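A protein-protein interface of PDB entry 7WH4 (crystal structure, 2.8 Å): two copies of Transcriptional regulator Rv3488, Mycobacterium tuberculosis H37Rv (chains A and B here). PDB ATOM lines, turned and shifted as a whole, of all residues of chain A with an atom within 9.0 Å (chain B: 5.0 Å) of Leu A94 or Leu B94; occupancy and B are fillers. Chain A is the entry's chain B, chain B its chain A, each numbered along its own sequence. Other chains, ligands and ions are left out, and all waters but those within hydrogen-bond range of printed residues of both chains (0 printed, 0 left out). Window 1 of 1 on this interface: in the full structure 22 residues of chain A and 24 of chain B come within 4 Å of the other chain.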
ATOM      1  N   PHE A   6     -21.885 -26.943  -9.116  1.00  0.00           N
ATOM      2  CA  PHE A   6     -21.692 -27.075  -7.684  1.00  0.00           C
ATOM      3  C   PHE A   6     -22.579 -26.079  -6.940  1.00  0.00           C
ATOM      4  O   PHE A   6     -23.303 -26.471  -6.033  1.00  0.00           O
ATOM      5  CB  PHE A   6     -20.221 -26.882  -7.303  1.00  0.00           C
ATOM      6  CG  PHE A   6     -20.018 -26.768  -5.813  1.00  0.00           C
ATOM      7  CD1 PHE A   6     -19.886 -27.906  -5.030  1.00  0.00           C
ATOM      8  CD2 PHE A   6     -20.014 -25.529  -5.185  1.00  0.00           C
ATOM      9  CE1 PHE A   6     -19.728 -27.809  -3.656  1.00  0.00           C
ATOM     10  CE2 PHE A   6     -19.854 -25.434  -3.811  1.00  0.00           C
ATOM     11  CZ  PHE A   6     -19.712 -26.572  -3.049  1.00  0.00           C
ATOM     12  N   MET A   7     -22.518 -24.797  -7.327  1.00  0.00           N
ATOM     13  CA  MET A   7     -23.233 -23.747  -6.619  1.00  0.00           C
ATOM     14  C   MET A   7     -24.743 -23.981  -6.689  1.00  0.00           C
ATOM     15  O   MET A   7     -25.457 -23.646  -5.751  1.00  0.00           O
ATOM     16  CB  MET A   7     -22.881 -22.352  -7.153  1.00  0.00           C
ATOM     17  CG  MET A   7     -21.462 -21.897  -6.814  1.00  0.00           C
ATOM     18  SD  MET A   7     -21.087 -21.721  -5.044  1.00  0.00           S
ATOM     19  CE  MET A   7     -21.788 -20.105  -4.708  1.00  0.00           C
ATOM     20  N   GLU A   9     -26.242 -27.007  -6.874  1.00  0.00           N
ATOM     21  CA  GLU A   9     -26.510 -28.095  -5.944  1.00  0.00           C
ATOM     22  C   GLU A   9     -26.305 -27.612  -4.506  1.00  0.00           C
ATOM     23  O   GLU A   9     -27.124 -27.897  -3.638  1.00  0.00           O
ATOM     24  CB  GLU A   9     -25.663 -29.330  -6.265  1.00  0.00           C
ATOM     25  N   PHE A  10     -25.218 -26.862  -4.273  1.00  0.00           N
ATOM     26  CA  PHE A  10     -24.871 -26.323  -2.963  1.00  0.00           C
ATOM     27  C   PHE A  10     -26.035 -25.518  -2.391  1.00  0.00           C
ATOM     28  O   PHE A  10     -26.308 -25.603  -1.199  1.00  0.00           O
ATOM     29  CB  PHE A  10     -23.599 -25.471  -3.044  1.00  0.00           C
ATOM     30  CG  PHE A  10     -23.271 -24.644  -1.827  1.00  0.00           C
ATOM     31  CD1 PHE A  10     -22.544 -25.184  -0.776  1.00  0.00           C
ATOM     32  CD2 PHE A  10     -23.664 -23.317  -1.744  1.00  0.00           C
ATOM     33  CE1 PHE A  10     -22.223 -24.415   0.334  1.00  0.00           C
ATOM     34  CE2 PHE A  10     -23.342 -22.548  -0.634  1.00  0.00           C
ATOM     35  CZ  PHE A  10     -22.622 -23.097   0.404  1.00  0.00           C
ATOM     36  N   GLN A  11     -26.715 -24.747  -3.252  1.00  0.00           N
ATOM     37  CA  GLN A  11     -27.838 -23.908  -2.864  1.00  0.00           C
ATOM     38  C   GLN A  11     -28.907 -24.746  -2.168  1.00  0.00           C
ATOM     39  O   GLN A  11     -29.467 -24.314  -1.164  1.00  0.00           O
ATOM     40  CB  GLN A  11     -28.439 -23.196  -4.082  1.00  0.00           C
ATOM     41  CG  GLN A  11     -28.796 -21.736  -3.828  1.00  0.00           C
ATOM     42  CD  GLN A  11     -27.587 -20.858  -3.598  1.00  0.00           C
ATOM     43  OE1 GLN A  11     -26.442 -21.267  -3.803  1.00  0.00           O
ATOM     44  NE2 GLN A  11     -27.833 -19.640  -3.139  1.00  0.00           N
ATOM     45  N   ALA A  13     -28.552 -27.734  -0.682  1.00  0.00           N
ATOM     46  CA  ALA A  13     -28.009 -28.202   0.584  1.00  0.00           C
ATOM     47  C   ALA A  13     -28.122 -27.112   1.646  1.00  0.00           C
ATOM     48  O   ALA A  13     -28.611 -27.369   2.740  1.00  0.00           O
ATOM     49  CB  ALA A  13     -26.575 -28.644   0.405  1.00  0.00           C
ATOM     50  N   ALA A  14     -27.673 -25.899   1.302  1.00  0.00           N
ATOM     51  CA  ALA A  14     -27.598 -24.781   2.229  1.00  0.00           C
ATOM     52  C   ALA A  14     -28.974 -24.462   2.805  1.00  0.00           C
ATOM     53  O   ALA A  14     -29.113 -24.324   4.022  1.00  0.00           O
ATOM     54  CB  ALA A  14     -26.998 -23.585   1.535  1.00  0.00           C
ATOM     55  N   LEU A  17     -30.202 -27.283   5.111  1.00  0.00           N
ATOM     56  CA  LEU A  17     -29.555 -27.376   6.408  1.00  0.00           C
ATOM     57  C   LEU A  17     -29.924 -26.172   7.269  1.00  0.00           C
ATOM     58  O   LEU A  17     -30.048 -26.306   8.485  1.00  0.00           O
ATOM     59  CB  LEU A  17     -28.045 -27.546   6.219  1.00  0.00           C
ATOM     60  CG  LEU A  17     -27.554 -28.994   6.088  1.00  0.00           C
ATOM     61  CD1 LEU A  17     -28.403 -29.811   5.119  1.00  0.00           C
ATOM     62  CD2 LEU A  17     -26.097 -29.033   5.656  1.00  0.00           C
ATOM     63  N   HIS A  18     -30.144 -25.016   6.629  1.00  0.00           N
ATOM     64  CA  HIS A  18     -30.534 -23.814   7.351  1.00  0.00           C
ATOM     65  C   HIS A  18     -31.930 -23.987   7.944  1.00  0.00           C
ATOM     66  O   HIS A  18     -32.163 -23.553   9.063  1.00  0.00           O
ATOM     67  CB  HIS A  18     -30.383 -22.553   6.488  1.00  0.00           C
ATOM     68  CG  HIS A  18     -29.045 -21.902   6.608  1.00  0.00           C
ATOM     69  ND1 HIS A  18     -28.703 -21.110   7.692  1.00  0.00           N
ATOM     70  CD2 HIS A  18     -27.967 -21.912   5.789  1.00  0.00           C
ATOM     71  CE1 HIS A  18     -27.473 -20.659   7.537  1.00  0.00           C
ATOM     72  NE2 HIS A  18     -26.996 -21.140   6.376  1.00  0.00           N
ATOM     73  N   TYR A  42     -29.101 -16.488   0.828  1.00  0.00           N
ATOM     74  CA  TYR A  42     -29.654 -17.572   0.028  1.00  0.00           C
ATOM     75  C   TYR A  42     -31.011 -17.169  -0.550  1.00  0.00           C
ATOM     76  O   TYR A  42     -31.981 -17.025   0.195  1.00  0.00           O
ATOM     77  CB  TYR A  42     -29.740 -18.855   0.863  1.00  0.00           C
ATOM     78  CG  TYR A  42     -28.425 -19.319   1.438  1.00  0.00           C
ATOM     79  CD1 TYR A  42     -27.471 -19.931   0.639  1.00  0.00           C
ATOM     80  CD2 TYR A  42     -28.132 -19.148   2.783  1.00  0.00           C
ATOM     81  CE1 TYR A  42     -26.257 -20.351   1.159  1.00  0.00           C
ATOM     82  CE2 TYR A  42     -26.931 -19.581   3.326  1.00  0.00           C
ATOM     83  CZ  TYR A  42     -25.991 -20.184   2.507  1.00  0.00           C
ATOM     84  OH  TYR A  42     -24.799 -20.623   3.006  1.00  0.00           O
ATOM     85  N   ALA A  86     -29.929 -35.632  11.642  1.00  0.00           N
ATOM     86  CA  ALA A  86     -29.643 -35.365  10.240  1.00  0.00           C
ATOM     87  C   ALA A  86     -28.755 -34.128  10.101  1.00  0.00           C
ATOM     88  O   ALA A  86     -27.731 -34.174   9.422  1.00  0.00           O
ATOM     89  CB  ALA A  86     -30.935 -35.221   9.470  1.00  0.00           C
ATOM     90  N   LEU A  87     -29.140 -33.033  10.771  1.00  0.00           N
ATOM     91  CA  LEU A  87     -28.369 -31.801  10.714  1.00  0.00           C
ATOM     92  C   LEU A  87     -26.907 -32.070  11.081  1.00  0.00           C
ATOM     93  O   LEU A  87     -26.004 -31.637  10.367  1.00  0.00           O
ATOM     94  CB  LEU A  87     -28.991 -30.741  11.629  1.00  0.00           C
ATOM     95  CG  LEU A  87     -28.261 -29.397  11.665  1.00  0.00           C
ATOM     96  CD1 LEU A  87     -28.453 -28.630  10.366  1.00  0.00           C
ATOM     97  CD2 LEU A  87     -28.736 -28.545  12.833  1.00  0.00           C
ATOM     98  N   THR A  88     -26.673 -32.784  12.191  1.00  0.00           N
ATOM     99  CA  THR A  88     -25.311 -32.979  12.672  1.00  0.00           C
ATOM    100  C   THR A  88     -24.543 -33.894  11.720  1.00  0.00           C
ATOM    101  O   THR A  88     -23.424 -33.562  11.344  1.00  0.00           O
ATOM    102  CB  THR A  88     -25.259 -33.375  14.153  1.00  0.00           C
ATOM    103  OG1 THR A  88     -25.778 -34.701  14.263  1.00  0.00           O
ATOM    104  CG2 THR A  88     -26.027 -32.431  15.057  1.00  0.00           C
ATOM    105  N   GLU A  89     -25.158 -35.016  11.315  1.00  0.00           N
ATOM    106  CA  GLU A  89     -24.564 -35.948  10.363  1.00  0.00           C
ATOM    107  C   GLU A  89     -24.161 -35.198   9.092  1.00  0.00           C
ATOM    108  O   GLU A  89     -23.057 -35.373   8.578  1.00  0.00           O
ATOM    109  CB  GLU A  89     -25.539 -37.079  10.004  1.00  0.00           C
ATOM    110  CG  GLU A  89     -25.211 -38.417  10.655  1.00  0.00           C
ATOM    111  N   ASP A  90     -25.074 -34.346   8.604  1.00  0.00           N
ATOM    112  CA  ASP A  90     -24.906 -33.605   7.363  1.00  0.00           C
ATOM    113  C   ASP A  90     -23.783 -32.574   7.510  1.00  0.00           C
ATOM    114  O   ASP A  90     -22.919 -32.465   6.638  1.00  0.00           O
ATOM    115  CB  ASP A  90     -26.235 -33.007   6.886  1.00  0.00           C
ATOM    116  CG  ASP A  90     -27.273 -34.024   6.417  1.00  0.00           C
ATOM    117  OD1 ASP A  90     -26.946 -35.229   6.352  1.00  0.00           O
ATOM    118  OD2 ASP A  90     -28.411 -33.606   6.118  1.00  0.00           O
ATOM    119  N   ARG A  91     -23.792 -31.821   8.619  1.00  0.00           N
ATOM    120  CA  ARG A  91     -22.763 -30.833   8.911  1.00  0.00           C
ATOM    121  C   ARG A  91     -21.385 -31.495   8.887  1.00  0.00           C
ATOM    122  O   ARG A  91     -20.466 -30.997   8.237  1.00  0.00           O
ATOM    123  CB  ARG A  91     -23.048 -30.146  10.254  1.00  0.00           C
ATOM    124  CG  ARG A  91     -22.195 -28.915  10.540  1.00  0.00           C
ATOM    125  CD  ARG A  91     -21.986 -28.720  12.043  1.00  0.00           C
ATOM    126  N   ARG A  92     -21.272 -32.638   9.580  1.00  0.00           N
ATOM    127  CA  ARG A  92     -20.041 -33.406   9.692  1.00  0.00           C
ATOM    128  C   ARG A  92     -19.554 -33.836   8.310  1.00  0.00           C
ATOM    129  O   ARG A  92     -18.361 -33.758   8.037  1.00  0.00           O
ATOM    130  CB  ARG A  92     -20.234 -34.614  10.620  1.00  0.00           C
ATOM    131  CG  ARG A  92     -19.869 -34.348  12.073  1.00  0.00           C
ATOM    132  N   ALA A  93     -20.484 -34.282   7.452  1.00  0.00           N
ATOM    133  CA  ALA A  93     -20.169 -34.762   6.113  1.00  0.00           C
ATOM    134  C   ALA A  93     -19.513 -33.654   5.291  1.00  0.00           C
ATOM    135  O   ALA A  93     -18.570 -33.909   4.547  1.00  0.00           O
ATOM    136  CB  ALA A  93     -21.416 -35.291   5.445  1.00  0.00           C
ATOM    137  N   LEU A  94     -20.023 -32.425   5.441  1.00  0.00           N
ATOM    138  CA  LEU A  94     -19.473 -31.260   4.769  1.00  0.00           C
ATOM    139  C   LEU A  94     -18.047 -31.006   5.254  1.00  0.00           C
ATOM    140  O   LEU A  94     -17.165 -30.719   4.449  1.00  0.00           O
ATOM    141  CB  LEU A  94     -20.369 -30.046   5.038  1.00  0.00           C
ATOM    142  CG  LEU A  94     -21.760 -30.081   4.406  1.00  0.00           C
ATOM    143  CD1 LEU A  94     -22.507 -28.796   4.717  1.00  0.00           C
ATOM    144  CD2 LEU A  94     -21.680 -30.282   2.898  1.00  0.00           C
ATOM    145  N   GLU A  95     -17.838 -31.131   6.571  1.00  0.00           N
ATOM    146  CA  GLU A  95     -16.551 -30.898   7.214  1.00  0.00           C
ATOM    147  C   GLU A  95     -15.509 -31.888   6.694  1.00  0.00           C
ATOM    148  O   GLU A  95     -14.386 -31.491   6.368  1.00  0.00           O
ATOM    149  CB  GLU A  95     -16.689 -30.976   8.737  1.00  0.00           C
ATOM    150  CG  GLU A  95     -17.182 -29.683   9.372  1.00  0.00           C
ATOM    151  CD  GLU A  95     -17.980 -29.841  10.660  1.00  0.00           C
ATOM    152  N   GLU A  96     -15.899 -33.171   6.604  1.00  0.00           N
ATOM    153  CA  GLU A  96     -15.023 -34.237   6.136  1.00  0.00           C
ATOM    154  C   GLU A  96     -14.627 -34.000   4.678  1.00  0.00           C
ATOM    155  O   GLU A  96     -13.479 -34.234   4.314  1.00  0.00           O
ATOM    156  CB  GLU A  96     -15.657 -35.625   6.311  1.00  0.00           C
ATOM    157  CG  GLU A  96     -15.335 -36.303   7.634  1.00  0.00           C
ATOM    158  N   LEU A  97     -15.573 -33.538   3.850  1.00  0.00           N
ATOM    159  CA  LEU A  97     -15.309 -33.371   2.428  1.00  0.00           C
ATOM    160  C   LEU A  97     -14.309 -32.236   2.224  1.00  0.00           C
ATOM    161  O   LEU A  97     -13.308 -32.420   1.535  1.00  0.00           O
ATOM    162  CB  LEU A  97     -16.620 -33.128   1.669  1.00  0.00           C
ATOM    163  CG  LEU A  97     -16.504 -32.991   0.147  1.00  0.00           C
ATOM    164  CD1 LEU A  97     -15.713 -34.140  -0.467  1.00  0.00           C
ATOM    165  CD2 LEU A  97     -17.880 -32.899  -0.495  1.00  0.00           C
ATOM    166  N   ALA A  98     -14.578 -31.081   2.849  1.00  0.00           N
ATOM    167  CA  ALA A  98     -13.731 -29.903   2.738  1.00  0.00           C
ATOM    168  C   ALA A  98     -12.282 -30.229   3.104  1.00  0.00           C
ATOM    169  O   ALA A  98     -11.358 -29.783   2.426  1.00  0.00           O
ATOM    170  CB  ALA A  98     -14.283 -28.784   3.588  1.00  0.00           C
ATOM    171  N   ARG A  99     -12.092 -31.011   4.177  1.00  0.00           N
ATOM    172  CA  ARG A  99     -10.770 -31.364   4.680  1.00  0.00           C
ATOM    173  C   ARG A  99     -10.085 -32.358   3.743  1.00  0.00           C
ATOM    174  O   ARG A  99      -8.874 -32.299   3.554  1.00  0.00           O
ATOM    175  CB  ARG A  99     -10.874 -31.921   6.104  1.00  0.00           C
ATOM    176  CG  ARG A  99     -11.015 -30.843   7.170  1.00  0.00           C
ATOM    177  CD  ARG A  99     -10.728 -31.342   8.574  1.00  0.00           C
ATOM    178  NE  ARG A  99     -11.935 -31.763   9.274  1.00  0.00           N
ATOM    179  CZ  ARG A  99     -12.755 -30.950   9.936  1.00  0.00           C
ATOM    180  NH1 ARG A  99     -13.823 -31.441  10.539  1.00  0.00           N
ATOM    181  NH2 ARG A  99     -12.511 -29.652   9.994  1.00  0.00           N
ATOM    182  N   GLU A 100     -10.883 -33.272   3.175  1.00  0.00           N
ATOM    183  CA  GLU A 100     -10.438 -34.333   2.286  1.00  0.00           C
ATOM    184  C   GLU A 100      -9.715 -33.739   1.077  1.00  0.00           C
ATOM    185  O   GLU A 100      -8.674 -34.254   0.664  1.00  0.00           O
ATOM    186  CB  GLU A 100     -11.644 -35.161   1.829  1.00  0.00           C
ATOM    187  CG  GLU A 100     -11.447 -36.670   1.905  1.00  0.00           C
ATOM    188  CD  GLU A 100     -12.689 -37.489   2.237  1.00  0.00           C
ATOM    189  OE1 GLU A 100     -13.225 -38.167   1.330  1.00  0.00           O
ATOM    190  OE2 GLU A 100     -13.108 -37.465   3.412  1.00  0.00           O
ATOM    191  N   VAL A 101     -10.261 -32.642   0.530  1.00  0.00           N
ATOM    192  CA  VAL A 101      -9.731 -32.020  -0.676  1.00  0.00           C
ATOM    193  C   VAL A 101      -8.823 -30.848  -0.292  1.00  0.00           C
ATOM    194  O   VAL A 101      -9.036 -29.714  -0.719  1.00  0.00           O
ATOM    195  CB  VAL A 101     -10.851 -31.613  -1.657  1.00  0.00           C
ATOM    196  CG1 VAL A 101     -11.579 -32.829  -2.208  1.00  0.00           C
ATOM    197  CG2 VAL A 101     -11.850 -30.638  -1.053  1.00  0.00           C
ATOM    198  N   PHE B   6     -30.186 -36.126   1.242  1.00  0.00           N
ATOM    199  CA  PHE B   6     -28.983 -35.310   1.240  1.00  0.00           C
ATOM    200  C   PHE B   6     -27.774 -36.144   0.816  1.00  0.00           C
ATOM    201  O   PHE B   6     -26.992 -35.716  -0.034  1.00  0.00           O
ATOM    202  CB  PHE B   6     -28.768 -34.674   2.614  1.00  0.00           C
ATOM    203  CG  PHE B   6     -27.385 -34.126   2.842  1.00  0.00           C
ATOM    204  CD1 PHE B   6     -26.360 -34.954   3.273  1.00  0.00           C
ATOM    205  CD2 PHE B   6     -27.102 -32.790   2.608  1.00  0.00           C
ATOM    206  CE1 PHE B   6     -25.081 -34.457   3.477  1.00  0.00           C
ATOM    207  CE2 PHE B   6     -25.824 -32.292   2.814  1.00  0.00           C
ATOM    208  CZ  PHE B   6     -24.816 -33.126   3.248  1.00  0.00           C
ATOM    209  N   PHE B  10     -25.147 -35.451  -1.936  1.00  0.00           N
ATOM    210  CA  PHE B  10     -23.812 -35.222  -1.401  1.00  0.00           C
ATOM    211  C   PHE B  10     -22.776 -36.086  -2.127  1.00  0.00           C
ATOM    212  O   PHE B  10     -21.677 -35.616  -2.430  1.00  0.00           O
ATOM    213  CB  PHE B  10     -23.774 -35.457   0.115  1.00  0.00           C
ATOM    214  CG  PHE B  10     -22.393 -35.439   0.731  1.00  0.00           C
ATOM    215  CD1 PHE B  10     -21.791 -34.245   1.107  1.00  0.00           C
ATOM    216  CD2 PHE B  10     -21.690 -36.619   0.936  1.00  0.00           C
ATOM    217  CE1 PHE B  10     -20.520 -34.232   1.662  1.00  0.00           C
ATOM    218  CE2 PHE B  10     -20.418 -36.604   1.490  1.00  0.00           C
ATOM    219  CZ  PHE B  10     -19.835 -35.411   1.854  1.00  0.00           C
ATOM    220  N   LEU B  17     -15.765 -33.142  -6.604  1.00  0.00           N
ATOM    221  CA  LEU B  17     -14.690 -32.381  -5.987  1.00  0.00           C
ATOM    222  C   LEU B  17     -13.414 -33.221  -5.890  1.00  0.00           C
ATOM    223  O   LEU B  17     -12.313 -32.680  -5.970  1.00  0.00           O
ATOM    224  CB  LEU B  17     -15.134 -31.876  -4.610  1.00  0.00           C
ATOM    225  CG  LEU B  17     -15.638 -30.435  -4.573  1.00  0.00           C
ATOM    226  CD1 LEU B  17     -16.924 -30.291  -5.371  1.00  0.00           C
ATOM    227  CD2 LEU B  17     -15.835 -29.960  -3.140  1.00  0.00           C
ATOM    228  N   ASP B  90     -15.219 -23.854  -4.008  1.00  0.00           N
ATOM    229  CA  ASP B  90     -16.158 -24.888  -3.597  1.00  0.00           C
ATOM    230  C   ASP B  90     -15.833 -25.383  -2.188  1.00  0.00           C
ATOM    231  O   ASP B  90     -16.730 -25.479  -1.356  1.00  0.00           O
ATOM    232  CB  ASP B  90     -16.210 -26.058  -4.591  1.00  0.00           C
ATOM    233  CG  ASP B  90     -16.868 -25.744  -5.925  1.00  0.00           C
ATOM    234  OD1 ASP B  90     -17.410 -24.626  -6.072  1.00  0.00           O
ATOM    235  OD2 ASP B  90     -16.832 -26.624  -6.811  1.00  0.00           O
ATOM    236  N   ARG B  91     -14.554 -25.698  -1.931  1.00  0.00           N
ATOM    237  CA  ARG B  91     -14.108 -26.170  -0.628  1.00  0.00           C
ATOM    238  C   ARG B  91     -14.504 -25.149   0.441  1.00  0.00           C
ATOM    239  O   ARG B  91     -15.076 -25.514   1.466  1.00  0.00           O
ATOM    240  CB  ARG B  91     -12.599 -26.446  -0.635  1.00  0.00           C
ATOM    241  CG  ARG B  91     -12.012 -26.826   0.717  1.00  0.00           C
ATOM    242  CD  ARG B  91     -10.537 -27.184   0.711  1.00  0.00           C
ATOM    243  NE  ARG B  91      -9.693 -26.483  -0.251  1.00  0.00           N
ATOM    244  CZ  ARG B  91      -9.188 -25.260  -0.097  1.00  0.00           C
ATOM    245  NH1 ARG B  91      -9.443 -24.558   0.997  1.00  0.00           N
ATOM    246  NH2 ARG B  91      -8.432 -24.740  -1.049  1.00  0.00           N
ATOM    247  N   ARG B  92     -14.204 -23.872   0.170  1.00  0.00           N
ATOM    248  CA  ARG B  92     -14.463 -22.775   1.090  1.00  0.00           C
ATOM    249  C   ARG B  92     -15.960 -22.666   1.389  1.00  0.00           C
ATOM    250  O   ARG B  92     -16.351 -22.473   2.542  1.00  0.00           O
ATOM    251  CB  ARG B  92     -13.834 -21.481   0.558  1.00  0.00           C
ATOM    252  CG  ARG B  92     -12.392 -21.272   1.011  1.00  0.00           C
ATOM    253  CD  ARG B  92     -11.430 -20.765  -0.050  1.00  0.00           C
ATOM    254  NE  ARG B  92     -10.045 -20.773   0.418  1.00  0.00           N
ATOM    255  CZ  ARG B  92      -9.254 -19.705   0.509  1.00  0.00           C
ATOM    256  NH1 ARG B  92      -9.696 -18.514   0.142  1.00  0.00           N
ATOM    257  NH2 ARG B  92      -8.016 -19.834   0.955  1.00  0.00           N
ATOM    258  N   ALA B  93     -16.789 -22.822   0.346  1.00  0.00           N
ATOM    259  CA  ALA B  93     -18.238 -22.732   0.454  1.00  0.00           C
ATOM    260  C   ALA B  93     -18.773 -23.793   1.415  1.00  0.00           C
ATOM    261  O   ALA B  93     -19.661 -23.501   2.219  1.00  0.00           O
ATOM    262  CB  ALA B  93     -18.878 -22.855  -0.909  1.00  0.00           C
ATOM    263  N   LEU B  94     -18.217 -25.013   1.318  1.00  0.00           N
ATOM    264  CA  LEU B  94     -18.579 -26.130   2.180  1.00  0.00           C
ATOM    265  C   LEU B  94     -18.242 -25.777   3.628  1.00  0.00           C
ATOM    266  O   LEU B  94     -19.032 -26.042   4.536  1.00  0.00           O
ATOM    267  CB  LEU B  94     -17.808 -27.388   1.757  1.00  0.00           C
ATOM    268  CG  LEU B  94     -18.169 -28.015   0.411  1.00  0.00           C
ATOM    269  CD1 LEU B  94     -17.367 -29.291   0.199  1.00  0.00           C
ATOM    270  CD2 LEU B  94     -19.660 -28.299   0.311  1.00  0.00           C
ATOM    271  N   GLU B  95     -17.054 -25.181   3.824  1.00  0.00           N
ATOM    272  CA  GLU B  95     -16.555 -24.804   5.136  1.00  0.00           C
ATOM    273  C   GLU B  95     -17.478 -23.777   5.783  1.00  0.00           C
ATOM    274  O   GLU B  95     -17.789 -23.907   6.962  1.00  0.00           O
ATOM    275  CB  GLU B  95     -15.145 -24.217   5.048  1.00  0.00           C
ATOM    276  CG  GLU B  95     -14.045 -25.255   5.035  1.00  0.00           C
ATOM    277  CD  GLU B  95     -12.724 -24.714   4.513  1.00  0.00           C
ATOM    278  OE1 GLU B  95     -12.495 -23.489   4.627  1.00  0.00           O
ATOM    279  OE2 GLU B  95     -11.929 -25.517   3.982  1.00  0.00           O
ATOM    280  N   GLU B  96     -17.897 -22.762   5.009  1.00  0.00           N
ATOM    281  CA  GLU B  96     -18.713 -21.679   5.533  1.00  0.00           C
ATOM    282  C   GLU B  96     -20.097 -22.194   5.917  1.00  0.00           C
ATOM    283  O   GLU B  96     -20.666 -21.750   6.913  1.00  0.00           O
ATOM    284  CB  GLU B  96     -18.781 -20.501   4.561  1.00  0.00           C
ATOM    285  CG  GLU B  96     -18.896 -19.171   5.285  1.00  0.00           C
ATOM    286  CD  GLU B  96     -17.994 -19.046   6.503  1.00  0.00           C
ATOM    287  OE1 GLU B  96     -16.759 -19.036   6.324  1.00  0.00           O
ATOM    288  OE2 GLU B  96     -18.526 -18.971   7.628  1.00  0.00           O
ATOM    289  N   LEU B  97     -20.627 -23.146   5.135  1.00  0.00           N
ATOM    290  CA  LEU B  97     -21.938 -23.712   5.425  1.00  0.00           C
ATOM    291  C   LEU B  97     -21.899 -24.484   6.746  1.00  0.00           C
ATOM    292  O   LEU B  97     -22.704 -24.218   7.639  1.00  0.00           O
ATOM    293  CB  LEU B  97     -22.412 -24.579   4.251  1.00  0.00           C
ATOM    294  CG  LEU B  97     -23.804 -25.200   4.389  1.00  0.00           C
ATOM    295  CD1 LEU B  97     -24.848 -24.155   4.753  1.00  0.00           C
ATOM    296  CD2 LEU B  97     -24.202 -25.926   3.112  1.00  0.00           C
ATOM    297  N   ALA B  98     -20.951 -25.422   6.867  1.00  0.00           N
ATOM    298  CA  ALA B  98     -20.806 -26.257   8.050  1.00  0.00           C
ATOM    299  C   ALA B  98     -20.671 -25.400   9.312  1.00  0.00           C
ATOM    300  O   ALA B  98     -21.266 -25.728  10.335  1.00  0.00           O
ATOM    301  CB  ALA B  98     -19.633 -27.191   7.883  1.00  0.00           C
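The backbone carbonyl oxygen (O) of Val A101 lies close to the guanidinium group (NE) of Arg B91.
Among the printed residues, merely in contact across the chains: Phe A6 with Leu B17, Phe A6 with Asp B90, Phe A6 with Leu B94, Phe A10 with Ala B93, Phe A10 with Leu B97, Ala A14 with Leu B97, His A18 with Leu B97, Tyr A42 with Leu B97, Asp A90 with Phe B6, Arg A91 with Ala B98, Ala A93 with Phe B10, Leu A94 with Leu B94, Leu A94 with Leu B97, Glu A95 with Ala B98, Leu A97 with Phe B10, Leu A97 with Leu B94, Ala A98 with Arg B91, Ala A98 with Glu B95 and Val A101 with Leu B17.
Of the printed residues of chain A, Leu B17 touches Phe A6 and Val A101.
Of the printed residues of chain B, Ala A14 touches Leu B97 (3.7 Å).
Printed residues of chain A within 4 Å of Asp B90: Phe A6.
Ala A13 touches none of the printed residues of chain B.
The nearest residue of chain A that does not touch Leu B94 is Phe A10 (4.2 Å).
Of the 12 printed residues of chain B, 10 touch a printed residue of chain A.
Hydrophobic or aromatic side chains of chain B within 4 Å of the printed part of chain A: Phe B6, Phe B10, Leu B17, Ala B93, Leu B94, Leu B97 and Ala B98.
Printed residues of chain A that touch a printed residue of chain B: Phe A6, Phe A10, Ala A14, His A18, Tyr A42, Asp A90, Arg A91, Ala A93, Leu A94, Glu A95, Leu A97, Ala A98 and Val A101.
Among the printed residues, 20 pairs touch across the chains.
Phe A6 touches Asp B90, and with the chains exchanged Asp A90 touches Phe B6.
Arg A91 touches Ala B98, and with the chains exchanged Ala A98 touches Arg B91.
Leu B94 touches its own counterpart, Leu A94.
Glu A95 touches Ala B98, and with the chains exchanged Ala A98 touches Glu B95.
12 positions are printed for both chains.
Of the 20 pairs that touch across the chains among the printed residues, 13 have their exchanged pair printed and touching as well.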
